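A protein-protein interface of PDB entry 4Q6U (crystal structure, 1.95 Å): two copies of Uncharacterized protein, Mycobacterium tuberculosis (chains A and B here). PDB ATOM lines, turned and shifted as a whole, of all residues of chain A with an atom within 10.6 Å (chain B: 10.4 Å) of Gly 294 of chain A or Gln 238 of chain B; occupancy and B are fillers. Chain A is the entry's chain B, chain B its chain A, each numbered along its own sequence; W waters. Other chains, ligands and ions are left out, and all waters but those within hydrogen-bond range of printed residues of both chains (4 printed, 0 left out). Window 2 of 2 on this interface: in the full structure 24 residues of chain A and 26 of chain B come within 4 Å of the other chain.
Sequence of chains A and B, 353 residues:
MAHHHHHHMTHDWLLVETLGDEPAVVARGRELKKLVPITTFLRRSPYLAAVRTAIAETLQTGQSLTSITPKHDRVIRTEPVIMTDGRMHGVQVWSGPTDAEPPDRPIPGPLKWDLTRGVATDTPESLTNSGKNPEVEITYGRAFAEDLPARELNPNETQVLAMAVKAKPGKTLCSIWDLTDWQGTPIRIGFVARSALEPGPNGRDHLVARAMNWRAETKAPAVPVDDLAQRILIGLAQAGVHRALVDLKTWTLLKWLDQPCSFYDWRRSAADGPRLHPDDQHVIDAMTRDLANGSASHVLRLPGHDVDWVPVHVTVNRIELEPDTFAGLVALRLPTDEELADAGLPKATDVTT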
ATOM      1  N   LEU A 248      30.436   3.488 -14.651  1.00  0.00           N
ATOM      2  CA  LEU A 248      30.762   2.140 -14.206  1.00  0.00           C
ATOM      3  C   LEU A 248      31.179   2.065 -12.733  1.00  0.00           C
ATOM      4  O   LEU A 248      30.756   1.166 -12.000  1.00  0.00           O
ATOM      5  CB  LEU A 248      31.864   1.572 -15.100  1.00  0.00           C
ATOM      6  CG  LEU A 248      31.359   1.226 -16.505  1.00  0.00           C
ATOM      7  CD1 LEU A 248      32.496   0.821 -17.439  1.00  0.00           C
ATOM      8  CD2 LEU A 248      30.315   0.117 -16.410  1.00  0.00           C
ATOM      9  N   GLY A 294      33.229  -7.826 -24.352  1.00  0.00           N
ATOM     10  CA  GLY A 294      32.503  -8.860 -23.635  1.00  0.00           C
ATOM     11  C   GLY A 294      31.489  -8.295 -22.658  1.00  0.00           C
ATOM     12  O   GLY A 294      31.850  -7.606 -21.702  1.00  0.00           O
ATOM     13  N   SER A 295      30.213  -8.582 -22.891  1.00  0.00           N
ATOM     14  CA  SER A 295      29.176  -8.116 -21.984  1.00  0.00           C
ATOM     15  C   SER A 295      29.134  -8.961 -20.720  1.00  0.00           C
ATOM     16  O   SER A 295      29.666 -10.077 -20.682  1.00  0.00           O
ATOM     17  CB  SER A 295      27.803  -8.123 -22.663  1.00  0.00           C
ATOM     18  OG  SER A 295      27.419  -9.430 -23.035  1.00  0.00           O
ATOM     19  N   ALA A 296      28.511  -8.405 -19.685  1.00  0.00           N
ATOM     20  CA  ALA A 296      28.262  -9.115 -18.435  1.00  0.00           C
ATOM     21  C   ALA A 296      26.800  -8.953 -18.049  1.00  0.00           C
ATOM     22  O   ALA A 296      26.229  -7.867 -18.180  1.00  0.00           O
ATOM     23  CB  ALA A 296      29.164  -8.595 -17.324  1.00  0.00           C
ATOM     24  N   SER A 297      26.194 -10.030 -17.567  1.00  0.00           N
ATOM     25  CA  SER A 297      24.785  -9.988 -17.216  1.00  0.00           C
ATOM     26  C   SER A 297      24.541 -10.494 -15.797  1.00  0.00           C
ATOM     27  O   SER A 297      25.169 -11.454 -15.344  1.00  0.00           O
ATOM     28  CB  SER A 297      23.969 -10.802 -18.218  1.00  0.00           C
ATOM     29  OG  SER A 297      22.597 -10.467 -18.134  1.00  0.00           O
ATOM     30  N   VAL A 314      19.978  -6.854 -15.622  1.00  0.00           N
ATOM     31  CA  VAL A 314      20.903  -5.870 -16.159  1.00  0.00           C
ATOM     32  C   VAL A 314      21.930  -6.524 -17.080  1.00  0.00           C
ATOM     33  O   VAL A 314      22.545  -7.525 -16.711  1.00  0.00           O
ATOM     34  CB  VAL A 314      21.628  -5.147 -15.019  1.00  0.00           C
ATOM     35  CG1 VAL A 314      22.712  -4.267 -15.553  1.00  0.00           C
ATOM     36  CG2 VAL A 314      20.635  -4.342 -14.183  1.00  0.00           C
ATOM     37  N   THR A 315      22.101  -5.965 -18.277  1.00  0.00           N
ATOM     38  CA  THR A 315      23.123  -6.431 -19.219  1.00  0.00           C
ATOM     39  C   THR A 315      24.045  -5.261 -19.579  1.00  0.00           C
ATOM     40  O   THR A 315      23.583  -4.197 -19.991  1.00  0.00           O
ATOM     41  CB  THR A 315      22.492  -7.038 -20.479  1.00  0.00           C
ATOM     42  OG1 THR A 315      21.722  -8.189 -20.113  1.00  0.00           O
ATOM     43  CG2 THR A 315      23.567  -7.446 -21.493  1.00  0.00           C
ATOM     44  N   VAL A 316      25.349  -5.458 -19.400  1.00  0.00           N
ATOM     45  CA  VAL A 316      26.297  -4.347 -19.390  1.00  0.00           C
ATOM     46  C   VAL A 316      27.419  -4.516 -20.396  1.00  0.00           C
ATOM     47  O   VAL A 316      28.057  -5.567 -20.448  1.00  0.00           O
ATOM     48  CB  VAL A 316      26.936  -4.175 -17.999  1.00  0.00           C
ATOM     49  CG1 VAL A 316      27.568  -2.802 -17.869  1.00  0.00           C
ATOM     50  CG2 VAL A 316      25.905  -4.366 -16.924  1.00  0.00           C
ATOM     51  N   ASN A 317      27.648  -3.476 -21.197  1.00  0.00           N
ATOM     52  CA  ASN A 317      28.791  -3.426 -22.105  1.00  0.00           C
ATOM     53  C   ASN A 317      29.633  -2.200 -21.792  1.00  0.00           C
ATOM     54  O   ASN A 317      29.109  -1.191 -21.347  1.00  0.00           O
ATOM     55  CB  ASN A 317      28.338  -3.398 -23.571  1.00  0.00           C
ATOM     56  CG  ASN A 317      27.772  -4.732 -24.040  1.00  0.00           C
ATOM     57  OD1 ASN A 317      28.476  -5.541 -24.641  1.00  0.00           O
ATOM     58  ND2 ASN A 317      26.495  -4.964 -23.768  1.00  0.00           N
ATOM     59  N   ARG A 318      30.939  -2.290 -22.014  1.00  0.00           N
ATOM     60  CA  ARG A 318      31.804  -1.133 -21.820  1.00  0.00           C
ATOM     61  C   ARG A 318      31.891  -0.316 -23.104  1.00  0.00           C
ATOM     62  O   ARG A 318      32.212  -0.858 -24.153  1.00  0.00           O
ATOM     63  CB  ARG A 318      33.199  -1.570 -21.388  1.00  0.00           C
ATOM     64  CG  ARG A 318      34.117  -0.420 -21.041  1.00  0.00           C
ATOM     65  CD  ARG A 318      35.449  -0.915 -20.492  1.00  0.00           C
ATOM     66  NE  ARG A 318      36.315  -1.443 -21.543  1.00  0.00           N
ATOM     67  CZ  ARG A 318      37.481  -2.038 -21.317  1.00  0.00           C
ATOM     68  NH1 ARG A 318      37.921  -2.188 -20.074  1.00  0.00           N
ATOM     69  NH2 ARG A 318      38.209  -2.484 -22.330  1.00  0.00           N
ATOM     70  N   ILE A 319      31.593   0.975 -23.013  1.00  0.00           N
ATOM     71  CA  ILE A 319      31.718   1.883 -24.146  1.00  0.00           C
ATOM     72  C   ILE A 319      32.911   2.814 -23.955  1.00  0.00           C
ATOM     73  O   ILE A 319      33.053   3.437 -22.912  1.00  0.00           O
ATOM     74  CB  ILE A 319      30.453   2.745 -24.335  1.00  0.00           C
ATOM     75  CG1 ILE A 319      29.187   1.888 -24.302  1.00  0.00           C
ATOM     76  CG2 ILE A 319      30.539   3.550 -25.619  1.00  0.00           C
ATOM     77  CD1 ILE A 319      29.215   0.690 -25.244  1.00  0.00           C
ATOM     78  N   ALA A 327      32.455   4.206 -20.334  1.00  0.00           N
ATOM     79  CA  ALA A 327      31.162   4.295 -19.674  1.00  0.00           C
ATOM     80  C   ALA A 327      30.454   2.970 -19.840  1.00  0.00           C
ATOM     81  O   ALA A 327      30.863   2.140 -20.662  1.00  0.00           O
ATOM     82  CB  ALA A 327      30.326   5.431 -20.250  1.00  0.00           C
ATOM     83  N   GLY A 328      29.397   2.754 -19.063  1.00  0.00           N
ATOM     84  CA  GLY A 328      28.647   1.512 -19.175  1.00  0.00           C
ATOM     85  C   GLY A 328      27.405   1.663 -20.031  1.00  0.00           C
ATOM     86  O   GLY A 328      26.614   2.583 -19.838  1.00  0.00           O
ATOM     87  N   LEU A 329      27.247   0.778 -21.008  1.00  0.00           N
ATOM     88  CA  LEU A 329      25.978   0.669 -21.698  1.00  0.00           C
ATOM     89  C   LEU A 329      25.186  -0.410 -20.987  1.00  0.00           C
ATOM     90  O   LEU A 329      25.572  -1.580 -20.996  1.00  0.00           O
ATOM     91  CB  LEU A 329      26.152   0.317 -23.174  1.00  0.00           C
ATOM     92  CG  LEU A 329      24.841  -0.094 -23.845  1.00  0.00           C
ATOM     93  CD1 LEU A 329      23.893   1.090 -23.899  1.00  0.00           C
ATOM     94  CD2 LEU A 329      25.072  -0.682 -25.226  1.00  0.00           C
ATOM     95  N   ARG B 151      33.238  -1.919 -40.640  1.00  0.00           N
ATOM     96  CA  ARG B 151      33.140  -1.174 -39.373  1.00  0.00           C
ATOM     97  C   ARG B 151      33.135   0.340 -39.496  1.00  0.00           C
ATOM     98  O   ARG B 151      32.263   0.994 -38.931  1.00  0.00           O
ATOM     99  CB  ARG B 151      34.245  -1.532 -38.396  1.00  0.00           C
ATOM    100  CG  ARG B 151      34.063  -0.645 -37.148  1.00  0.00           C
ATOM    101  CD  ARG B 151      34.643  -1.165 -35.899  1.00  0.00           C
ATOM    102  NE  ARG B 151      34.004  -2.383 -35.433  1.00  0.00           N
ATOM    103  CZ  ARG B 151      34.436  -3.035 -34.366  1.00  0.00           C
ATOM    104  NH1 ARG B 151      35.474  -2.548 -33.704  1.00  0.00           N
ATOM    105  NH2 ARG B 151      33.858  -4.165 -33.972  1.00  0.00           N
ATOM    106  N   ILE B 232      29.014   3.605 -29.237  1.00  0.00           N
ATOM    107  CA  ILE B 232      28.146   2.656 -28.550  1.00  0.00           C
ATOM    108  C   ILE B 232      28.046   1.374 -29.377  1.00  0.00           C
ATOM    109  O   ILE B 232      28.114   0.260 -28.854  1.00  0.00           O
ATOM    110  CB  ILE B 232      26.752   3.246 -28.320  1.00  0.00           C
ATOM    111  CG1 ILE B 232      26.841   4.427 -27.335  1.00  0.00           C
ATOM    112  CG2 ILE B 232      25.795   2.193 -27.784  1.00  0.00           C
ATOM    113  CD1 ILE B 232      25.609   5.303 -27.335  1.00  0.00           C
ATOM    114  N   LEU B 233      27.918   1.550 -30.682  1.00  0.00           N
ATOM    115  CA  LEU B 233      27.804   0.418 -31.589  1.00  0.00           C
ATOM    116  C   LEU B 233      29.056  -0.447 -31.504  1.00  0.00           C
ATOM    117  O   LEU B 233      28.981  -1.676 -31.511  1.00  0.00           O
ATOM    118  CB  LEU B 233      27.575   0.913 -33.019  1.00  0.00           C
ATOM    119  CG  LEU B 233      26.705   0.079 -33.953  1.00  0.00           C
ATOM    120  CD1 LEU B 233      25.374  -0.280 -33.288  1.00  0.00           C
ATOM    121  CD2 LEU B 233      26.486   0.867 -35.249  1.00  0.00           C
ATOM    122  N   ILE B 234      30.212   0.201 -31.423  1.00  0.00           N
ATOM    123  CA  ILE B 234      31.479  -0.512 -31.312  1.00  0.00           C
ATOM    124  C   ILE B 234      31.577  -1.260 -29.976  1.00  0.00           C
ATOM    125  O   ILE B 234      32.005  -2.414 -29.932  1.00  0.00           O
ATOM    126  CB  ILE B 234      32.667   0.453 -31.472  1.00  0.00           C
ATOM    127  CG1 ILE B 234      32.787   0.897 -32.936  1.00  0.00           C
ATOM    128  CG2 ILE B 234      33.953  -0.193 -31.009  1.00  0.00           C
ATOM    129  CD1 ILE B 234      33.694   2.109 -33.172  1.00  0.00           C
ATOM    130  N   GLY B 235      31.164  -0.616 -28.886  1.00  0.00           N
ATOM    131  CA  GLY B 235      31.147  -1.276 -27.594  1.00  0.00           C
ATOM    132  C   GLY B 235      30.233  -2.496 -27.535  1.00  0.00           C
ATOM    133  O   GLY B 235      30.352  -3.313 -26.629  1.00  0.00           O
ATOM    134  N   LEU B 236      29.305  -2.611 -28.477  1.00  0.00           N
ATOM    135  CA  LEU B 236      28.392  -3.756 -28.508  1.00  0.00           C
ATOM    136  C   LEU B 236      28.989  -4.960 -29.248  1.00  0.00           C
ATOM    137  O   LEU B 236      28.329  -5.992 -29.419  1.00  0.00           O
ATOM    138  CB  LEU B 236      27.065  -3.350 -29.157  1.00  0.00           C
ATOM    139  CG  LEU B 236      26.067  -2.659 -28.220  1.00  0.00           C
ATOM    140  CD1 LEU B 236      24.955  -1.951 -28.978  1.00  0.00           C
ATOM    141  CD2 LEU B 236      25.487  -3.675 -27.222  1.00  0.00           C
ATOM    142  N   ALA B 237      30.234  -4.825 -29.699  1.00  0.00           N
ATOM    143  CA  ALA B 237      30.910  -5.918 -30.396  1.00  0.00           C
ATOM    144  C   ALA B 237      31.147  -7.068 -29.426  1.00  0.00           C
ATOM    145  O   ALA B 237      31.389  -6.849 -28.240  1.00  0.00           O
ATOM    146  CB  ALA B 237      32.222  -5.444 -31.002  1.00  0.00           C
ATOM    147  N   GLN B 238      31.054  -8.296 -29.920  1.00  0.00           N
ATOM    148  CA  GLN B 238      31.177  -9.466 -29.046  1.00  0.00           C
ATOM    149  C   GLN B 238      32.080 -10.472 -29.742  1.00  0.00           C
ATOM    150  O   GLN B 238      31.916 -10.712 -30.934  1.00  0.00           O
ATOM    151  CB  GLN B 238      29.804 -10.079 -28.762  1.00  0.00           C
ATOM    152  CG  GLN B 238      29.716 -10.928 -27.509  1.00  0.00           C
ATOM    153  CD  GLN B 238      29.208 -10.133 -26.317  1.00  0.00           C
ATOM    154  OE1 GLN B 238      29.982  -9.711 -25.458  1.00  0.00           O
ATOM    155  NE2 GLN B 238      27.898  -9.921 -26.267  1.00  0.00           N
ATOM    156  N   ALA B 239      33.036 -11.034 -29.014  1.00  0.00           N
ATOM    157  CA  ALA B 239      33.954 -12.020 -29.575  1.00  0.00           C
ATOM    158  C   ALA B 239      33.175 -13.167 -30.194  1.00  0.00           C
ATOM    159  O   ALA B 239      32.222 -13.657 -29.601  1.00  0.00           O
ATOM    160  CB  ALA B 239      34.900 -12.539 -28.508  1.00  0.00           C
ATOM    161  N   GLY B 240      33.565 -13.581 -31.396  1.00  0.00           N
ATOM    162  CA  GLY B 240      32.904 -14.698 -32.054  1.00  0.00           C
ATOM    163  C   GLY B 240      31.604 -14.334 -32.752  1.00  0.00           C
ATOM    164  O   GLY B 240      30.983 -15.179 -33.408  1.00  0.00           O
ATOM    165  N   VAL B 241      31.195 -13.070 -32.616  1.00  0.00           N
ATOM    166  CA  VAL B 241      29.965 -12.597 -33.220  1.00  0.00           C
ATOM    167  C   VAL B 241      30.327 -11.561 -34.271  1.00  0.00           C
ATOM    168  O   VAL B 241      31.104 -10.643 -33.992  1.00  0.00           O
ATOM    169  CB  VAL B 241      29.014 -11.981 -32.183  1.00  0.00           C
ATOM    170  CG1 VAL B 241      27.799 -11.377 -32.862  1.00  0.00           C
ATOM    171  CG2 VAL B 241      28.604 -13.032 -31.143  1.00  0.00           C
ATOM    172  N   HIS B 242      29.777 -11.712 -35.470  1.00  0.00           N
ATOM    173  CA  HIS B 242      30.111 -10.806 -36.573  1.00  0.00           C
ATOM    174  C   HIS B 242      28.851 -10.154 -37.103  1.00  0.00           C
ATOM    175  O   HIS B 242      27.958 -10.841 -37.598  1.00  0.00           O
ATOM    176  CB  HIS B 242      30.846 -11.567 -37.679  1.00  0.00           C
ATOM    177  CG  HIS B 242      32.077 -12.271 -37.201  1.00  0.00           C
ATOM    178  ND1 HIS B 242      33.349 -11.804 -37.453  1.00  0.00           N
ATOM    179  CD2 HIS B 242      32.230 -13.398 -36.463  1.00  0.00           C
ATOM    180  CE1 HIS B 242      34.233 -12.609 -36.893  1.00  0.00           C
ATOM    181  NE2 HIS B 242      33.578 -13.585 -36.286  1.00  0.00           N
ATOM    182  N   ARG B 243      28.768  -8.832 -36.983  1.00  0.00           N
ATOM    183  CA  ARG B 243      27.561  -8.105 -37.368  1.00  0.00           C
ATOM    184  C   ARG B 243      27.666  -7.515 -38.765  1.00  0.00           C
ATOM    185  O   ARG B 243      28.731  -7.017 -39.175  1.00  0.00           O
ATOM    186  CB  ARG B 243      27.253  -6.977 -36.369  1.00  0.00           C
ATOM    187  CG  ARG B 243      26.892  -7.462 -34.968  1.00  0.00           C
ATOM    188  CD  ARG B 243      26.915  -6.304 -33.955  1.00  0.00           C
ATOM    189  NE  ARG B 243      28.251  -5.713 -33.832  1.00  0.00           N
ATOM    190  CZ  ARG B 243      28.499  -4.561 -33.206  1.00  0.00           C
ATOM    191  NH1 ARG B 243      27.507  -3.883 -32.654  1.00  0.00           N
ATOM    192  NH2 ARG B 243      29.736  -4.094 -33.129  1.00  0.00           N
ATOM    193  N   LEU B 257      29.893  -4.690 -40.039  1.00  0.00           N
ATOM    194  CA  LEU B 257      30.047  -3.724 -38.957  1.00  0.00           C
ATOM    195  C   LEU B 257      31.186  -4.138 -38.033  1.00  0.00           C
ATOM    196  O   LEU B 257      31.732  -3.325 -37.289  1.00  0.00           O
ATOM    197  CB  LEU B 257      28.732  -3.586 -38.174  1.00  0.00           C
ATOM    198  CG  LEU B 257      27.547  -3.098 -39.006  1.00  0.00           C
ATOM    199  CD1 LEU B 257      26.314  -3.013 -38.148  1.00  0.00           C
ATOM    200  CD2 LEU B 257      27.846  -1.719 -39.638  1.00  0.00           C
ATOM    201  N   ASP B 258      31.530  -5.418 -38.090  1.00  0.00           N
ATOM    202  CA  ASP B 258      32.712  -5.954 -37.445  1.00  0.00           C
ATOM    203  C   ASP B 258      33.555  -6.499 -38.571  1.00  0.00           C
ATOM    204  O   ASP B 258      33.214  -6.300 -39.735  1.00  0.00           O
ATOM    205  CB  ASP B 258      32.355  -7.054 -36.433  1.00  0.00           C
ATOM    206  CG  ASP B 258      31.383  -6.564 -35.381  1.00  0.00           C
ATOM    207  OD1 ASP B 258      31.664  -5.490 -34.826  1.00  0.00           O
ATOM    208  OD2 ASP B 258      30.341  -7.216 -35.135  1.00  0.00           O
ATOM    209  N   GLN B 259      34.642  -7.183 -38.247  1.00  0.00           N
ATOM    210  CA  GLN B 259      35.419  -7.826 -39.295  1.00  0.00           C
ATOM    211  C   GLN B 259      34.602  -9.007 -39.809  1.00  0.00           C
ATOM    212  O   GLN B 259      33.841  -9.608 -39.048  1.00  0.00           O
ATOM    213  CB  GLN B 259      36.794  -8.276 -38.783  1.00  0.00           C
ATOM    214  CG  GLN B 259      37.722  -7.127 -38.408  1.00  0.00           C
ATOM    215  CD  GLN B 259      37.767  -6.027 -39.462  1.00  0.00           C
ATOM    216  OE1 GLN B 259      38.074  -6.277 -40.633  1.00  0.00           O
ATOM    217  NE2 GLN B 259      37.458  -4.800 -39.047  1.00  0.00           N
ATOM    218  N   PRO B 260      34.737  -9.327 -41.102  1.00  0.00           N
ATOM    219  CA  PRO B 260      33.950 -10.430 -41.663  1.00  0.00           C
ATOM    220  C   PRO B 260      34.309 -11.769 -41.037  1.00  0.00           C
ATOM    221  O   PRO B 260      35.409 -11.934 -40.510  1.00  0.00           O
ATOM    222  CB  PRO B 260      34.309 -10.400 -43.157  1.00  0.00           C
ATOM    223  CG  PRO B 260      35.549  -9.582 -43.258  1.00  0.00           C
ATOM    224  CD  PRO B 260      35.513  -8.615 -42.130  1.00  0.00           C
ATOM    225  N   CYS B 261      33.381 -12.718 -41.079  1.00  0.00           N
ATOM    226  CA  CYS B 261      33.632 -14.024 -40.480  1.00  0.00           C
ATOM    227  C   CYS B 261      34.134 -15.022 -41.513  1.00  0.00           C
ATOM    228  O   CYS B 261      33.934 -14.840 -42.714  1.00  0.00           O
ATOM    229  CB  CYS B 261      32.368 -14.558 -39.821  1.00  0.00           C
ATOM    230  SG  CYS B 261      31.062 -14.887 -40.990  1.00  0.00           S
ATOM    231  N   PHE B 263      33.660 -18.590 -41.043  1.00  0.00           N
ATOM    232  CA  PHE B 263      33.047 -19.909 -40.935  1.00  0.00           C
ATOM    233  C   PHE B 263      31.962 -20.181 -41.980  1.00  0.00           C
ATOM    234  O   PHE B 263      31.381 -21.263 -41.990  1.00  0.00           O
ATOM    235  CB  PHE B 263      32.489 -20.147 -39.522  1.00  0.00           C
ATOM    236  CG  PHE B 263      31.790 -18.957 -38.907  1.00  0.00           C
ATOM    237  CD1 PHE B 263      30.480 -18.649 -39.242  1.00  0.00           C
ATOM    238  CD2 PHE B 263      32.434 -18.180 -37.948  1.00  0.00           C
ATOM    239  CE1 PHE B 263      29.835 -17.557 -38.653  1.00  0.00           C
ATOM    240  CE2 PHE B 263      31.798 -17.102 -37.362  1.00  0.00           C
ATOM    241  CZ  PHE B 263      30.499 -16.790 -37.714  1.00  0.00           C
ATOM    242  N   THR B 315      20.765 -13.478 -35.483  1.00  0.00           N
ATOM    243  CA  THR B 315      19.851 -12.593 -34.784  1.00  0.00           C
ATOM    244  C   THR B 315      19.585 -11.390 -35.683  1.00  0.00           C
ATOM    245  O   THR B 315      20.519 -10.725 -36.106  1.00  0.00           O
ATOM    246  CB  THR B 315      20.437 -12.129 -33.440  1.00  0.00           C
ATOM    247  OG1 THR B 315      20.876 -13.272 -32.698  1.00  0.00           O
ATOM    248  CG2 THR B 315      19.406 -11.347 -32.628  1.00  0.00           C
ATOM    249  N   VAL B 330      22.113  -8.102 -39.015  1.00  0.00           N
ATOM    250  CA  VAL B 330      22.254  -9.490 -38.559  1.00  0.00           C
ATOM    251  C   VAL B 330      23.510  -9.694 -37.719  1.00  0.00           C
ATOM    252  O   VAL B 330      24.582  -9.163 -38.022  1.00  0.00           O
ATOM    253  CB  VAL B 330      22.256 -10.497 -39.739  1.00  0.00           C
ATOM    254  CG1 VAL B 330      20.981 -10.347 -40.533  1.00  0.00           C
ATOM    255  CG2 VAL B 330      23.485 -10.313 -40.634  1.00  0.00           C
ATOM    256  N   ALA B 331      23.352 -10.427 -36.625  1.00  0.00           N
ATOM    257  CA  ALA B 331      24.481 -10.849 -35.809  1.00  0.00           C
ATOM    258  C   ALA B 331      24.717 -12.318 -36.105  1.00  0.00           C
ATOM    259  O   ALA B 331      23.829 -13.134 -35.883  1.00  0.00           O
ATOM    260  CB  ALA B 331      24.200 -10.641 -34.302  1.00  0.00           C
ATOM    261  N   LEU B 332      25.904 -12.646 -36.601  1.00  0.00           N
ATOM    262  CA  LEU B 332      26.214 -14.000 -37.058  1.00  0.00           C
ATOM    263  C   LEU B 332      27.215 -14.657 -36.138  1.00  0.00           C
ATOM    264  O   LEU B 332      28.265 -14.082 -35.844  1.00  0.00           O
ATOM    265  CB  LEU B 332      26.774 -13.970 -38.490  1.00  0.00           C
ATOM    266  CG  LEU B 332      25.923 -13.266 -39.544  1.00  0.00           C
ATOM    267  CD1 LEU B 332      26.772 -12.880 -40.757  1.00  0.00           C
ATOM    268  CD2 LEU B 332      24.765 -14.149 -39.963  1.00  0.00           C
ATOM    269  N   ARG B 333      26.897 -15.864 -35.683  1.00  0.00           N
ATOM    270  CA  ARG B 333      27.836 -16.631 -34.881  1.00  0.00           C
ATOM    271  C   ARG B 333      27.597 -18.133 -35.037  1.00  0.00           C
ATOM    272  O   ARG B 333      26.542 -18.566 -35.502  1.00  0.00           O
ATOM    273  CB  ARG B 333      27.739 -16.241 -33.404  1.00  0.00           C
ATOM    274  CG  ARG B 333      26.403 -16.573 -32.756  1.00  0.00           C
ATOM    275  CD  ARG B 333      26.500 -16.519 -31.239  1.00  0.00           C
ATOM    276  NE  ARG B 333      25.191 -16.556 -30.594  1.00  0.00           N
ATOM    277  CZ  ARG B 333      24.511 -17.669 -30.352  1.00  0.00           C
ATOM    278  NH1 ARG B 333      25.009 -18.848 -30.719  1.00  0.00           N
ATOM    279  NH2 ARG B 333      23.329 -17.605 -29.752  1.00  0.00           N
ATOM    280  N   LEU B 334      28.589 -18.923 -34.650  1.00  0.00           N
ATOM    281  CA  LEU B 334      28.436 -20.376 -34.652  1.00  0.00           C
ATOM    282  C   LEU B 334      27.304 -20.781 -33.715  1.00  0.00           C
ATOM    283  O   LEU B 334      27.161 -20.212 -32.639  1.00  0.00           O
ATOM    284  CB  LEU B 334      29.748 -21.051 -34.243  1.00  0.00           C
ATOM    285  CG  LEU B 334      30.892 -20.902 -35.252  1.00  0.00           C
ATOM    286  CD1 LEU B 334      32.211 -21.454 -34.724  1.00  0.00           C
ATOM    287  CD2 LEU B 334      30.522 -21.581 -36.563  1.00  0.00           C
HETATM  288  O   HOH W   1      33.744  -9.896 -26.406  1.00  0.00           O
HETATM  289  O   HOH W   2      25.516  -9.226 -24.809  1.00  0.00           O
HETATM  290  O   HOH W   3      30.665 -11.503 -22.726  1.00  0.00           O
HETATM  291  O   HOH W   4      33.360  -3.288 -25.215  1.00  0.00           O
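The backbone NH (N) of Ser 295 of chain A sits at hydrogen-bond distance from the side-chain amide oxygen (OE1) of Gln 238 of chain B, at 2.8 Å.
The backbone carbonyl oxygen of Asn 317 of chain A sits at hydrogen-bond distance from the backbone NH of Leu 329 of chain A. The backbone NH (N) of Ile 319 of chain A is in hydrogen-bond range of the backbone carbonyl oxygen (O) of Ala 327 of chain A (2.7 Å).
Among the printed residues, pairs that only touch across the chains: Gly 294 of chain A with Gln 238 of chain B (3.2 Å), Asn 317 of chain A with Gly 235 of chain B (3.5 Å), Asn 317 of chain A with Leu 236 of chain B (3.8 Å), Arg 318 of chain A with Gly 235 of chain B (3.6 Å), Ile 319 of chain A with Ile 232 of chain B (3.8 Å), Ile 319 of chain A with Gly 235 of chain B (3.6 Å), Leu 329 of chain A with Ile 232 of chain B (3.9 Å) and Leu 329 of chain A with Leu 236 of chain B (3.6 Å).
Printed residues of chain B within 4 Å of Gly 294 of chain A: Gln 238. Gln 238 of chain B touches two residues of chain A. Of chain B, only Gln 238 comes within 4 Å of Ser 295 of chain A. Ala 237 of chain B touches none of the printed residues of chain A. Ala 239 of chain B touches none of the printed residues of chain A. No residue of chain A comes within 4 Å of Val 241 of chain B. Of the printed residues of chain A, Leu 236 of chain B touches Asn 317 (3.8 Å) and Leu 329 (3.6 Å). Of the printed residues of chain B, Leu 329 of chain A touches Ile 232 (3.9 Å) and Leu 236 (3.6 Å). Ala 331 of chain B touches none of the printed residues of chain A. The nearest residue of chain A that does not touch Gln 238 of chain B is Asn 317 of chain A (4.5 Å). The nearest printed residue of chain B that does not touch Asn 317 of chain A is Gln 238 of chain B (4.5 Å).
Hydrophobic or aromatic side chains of chain B that line the printed part of chain A: Ile 232 and Leu 236.
Position printed for both chains: 315.
Water W2 lies within hydrogen-bond range of OG of Ser 295 of chain A (2.6 Å) and NE2 of Gln 238 of chain B (2.9 Å). Water W3 bridges the backbone carbonyl oxygen (O) of Ser 295 of chain A (2.7 Å) and the side-chain amide oxygen (OE1) of Gln 238 of chain B (3.3 Å). Water W4 bridges the backbone carbonyl oxygen of Arg 318 of chain A (2.9 Å) and the backbone carbonyl oxygen of Gly 235 of chain B (3.3 Å). Water W1 bridges the backbone NH of Ala 239 of chain B (2.9 Å) and the backbone NH of Gly 294 of chain A (3.0 Å).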
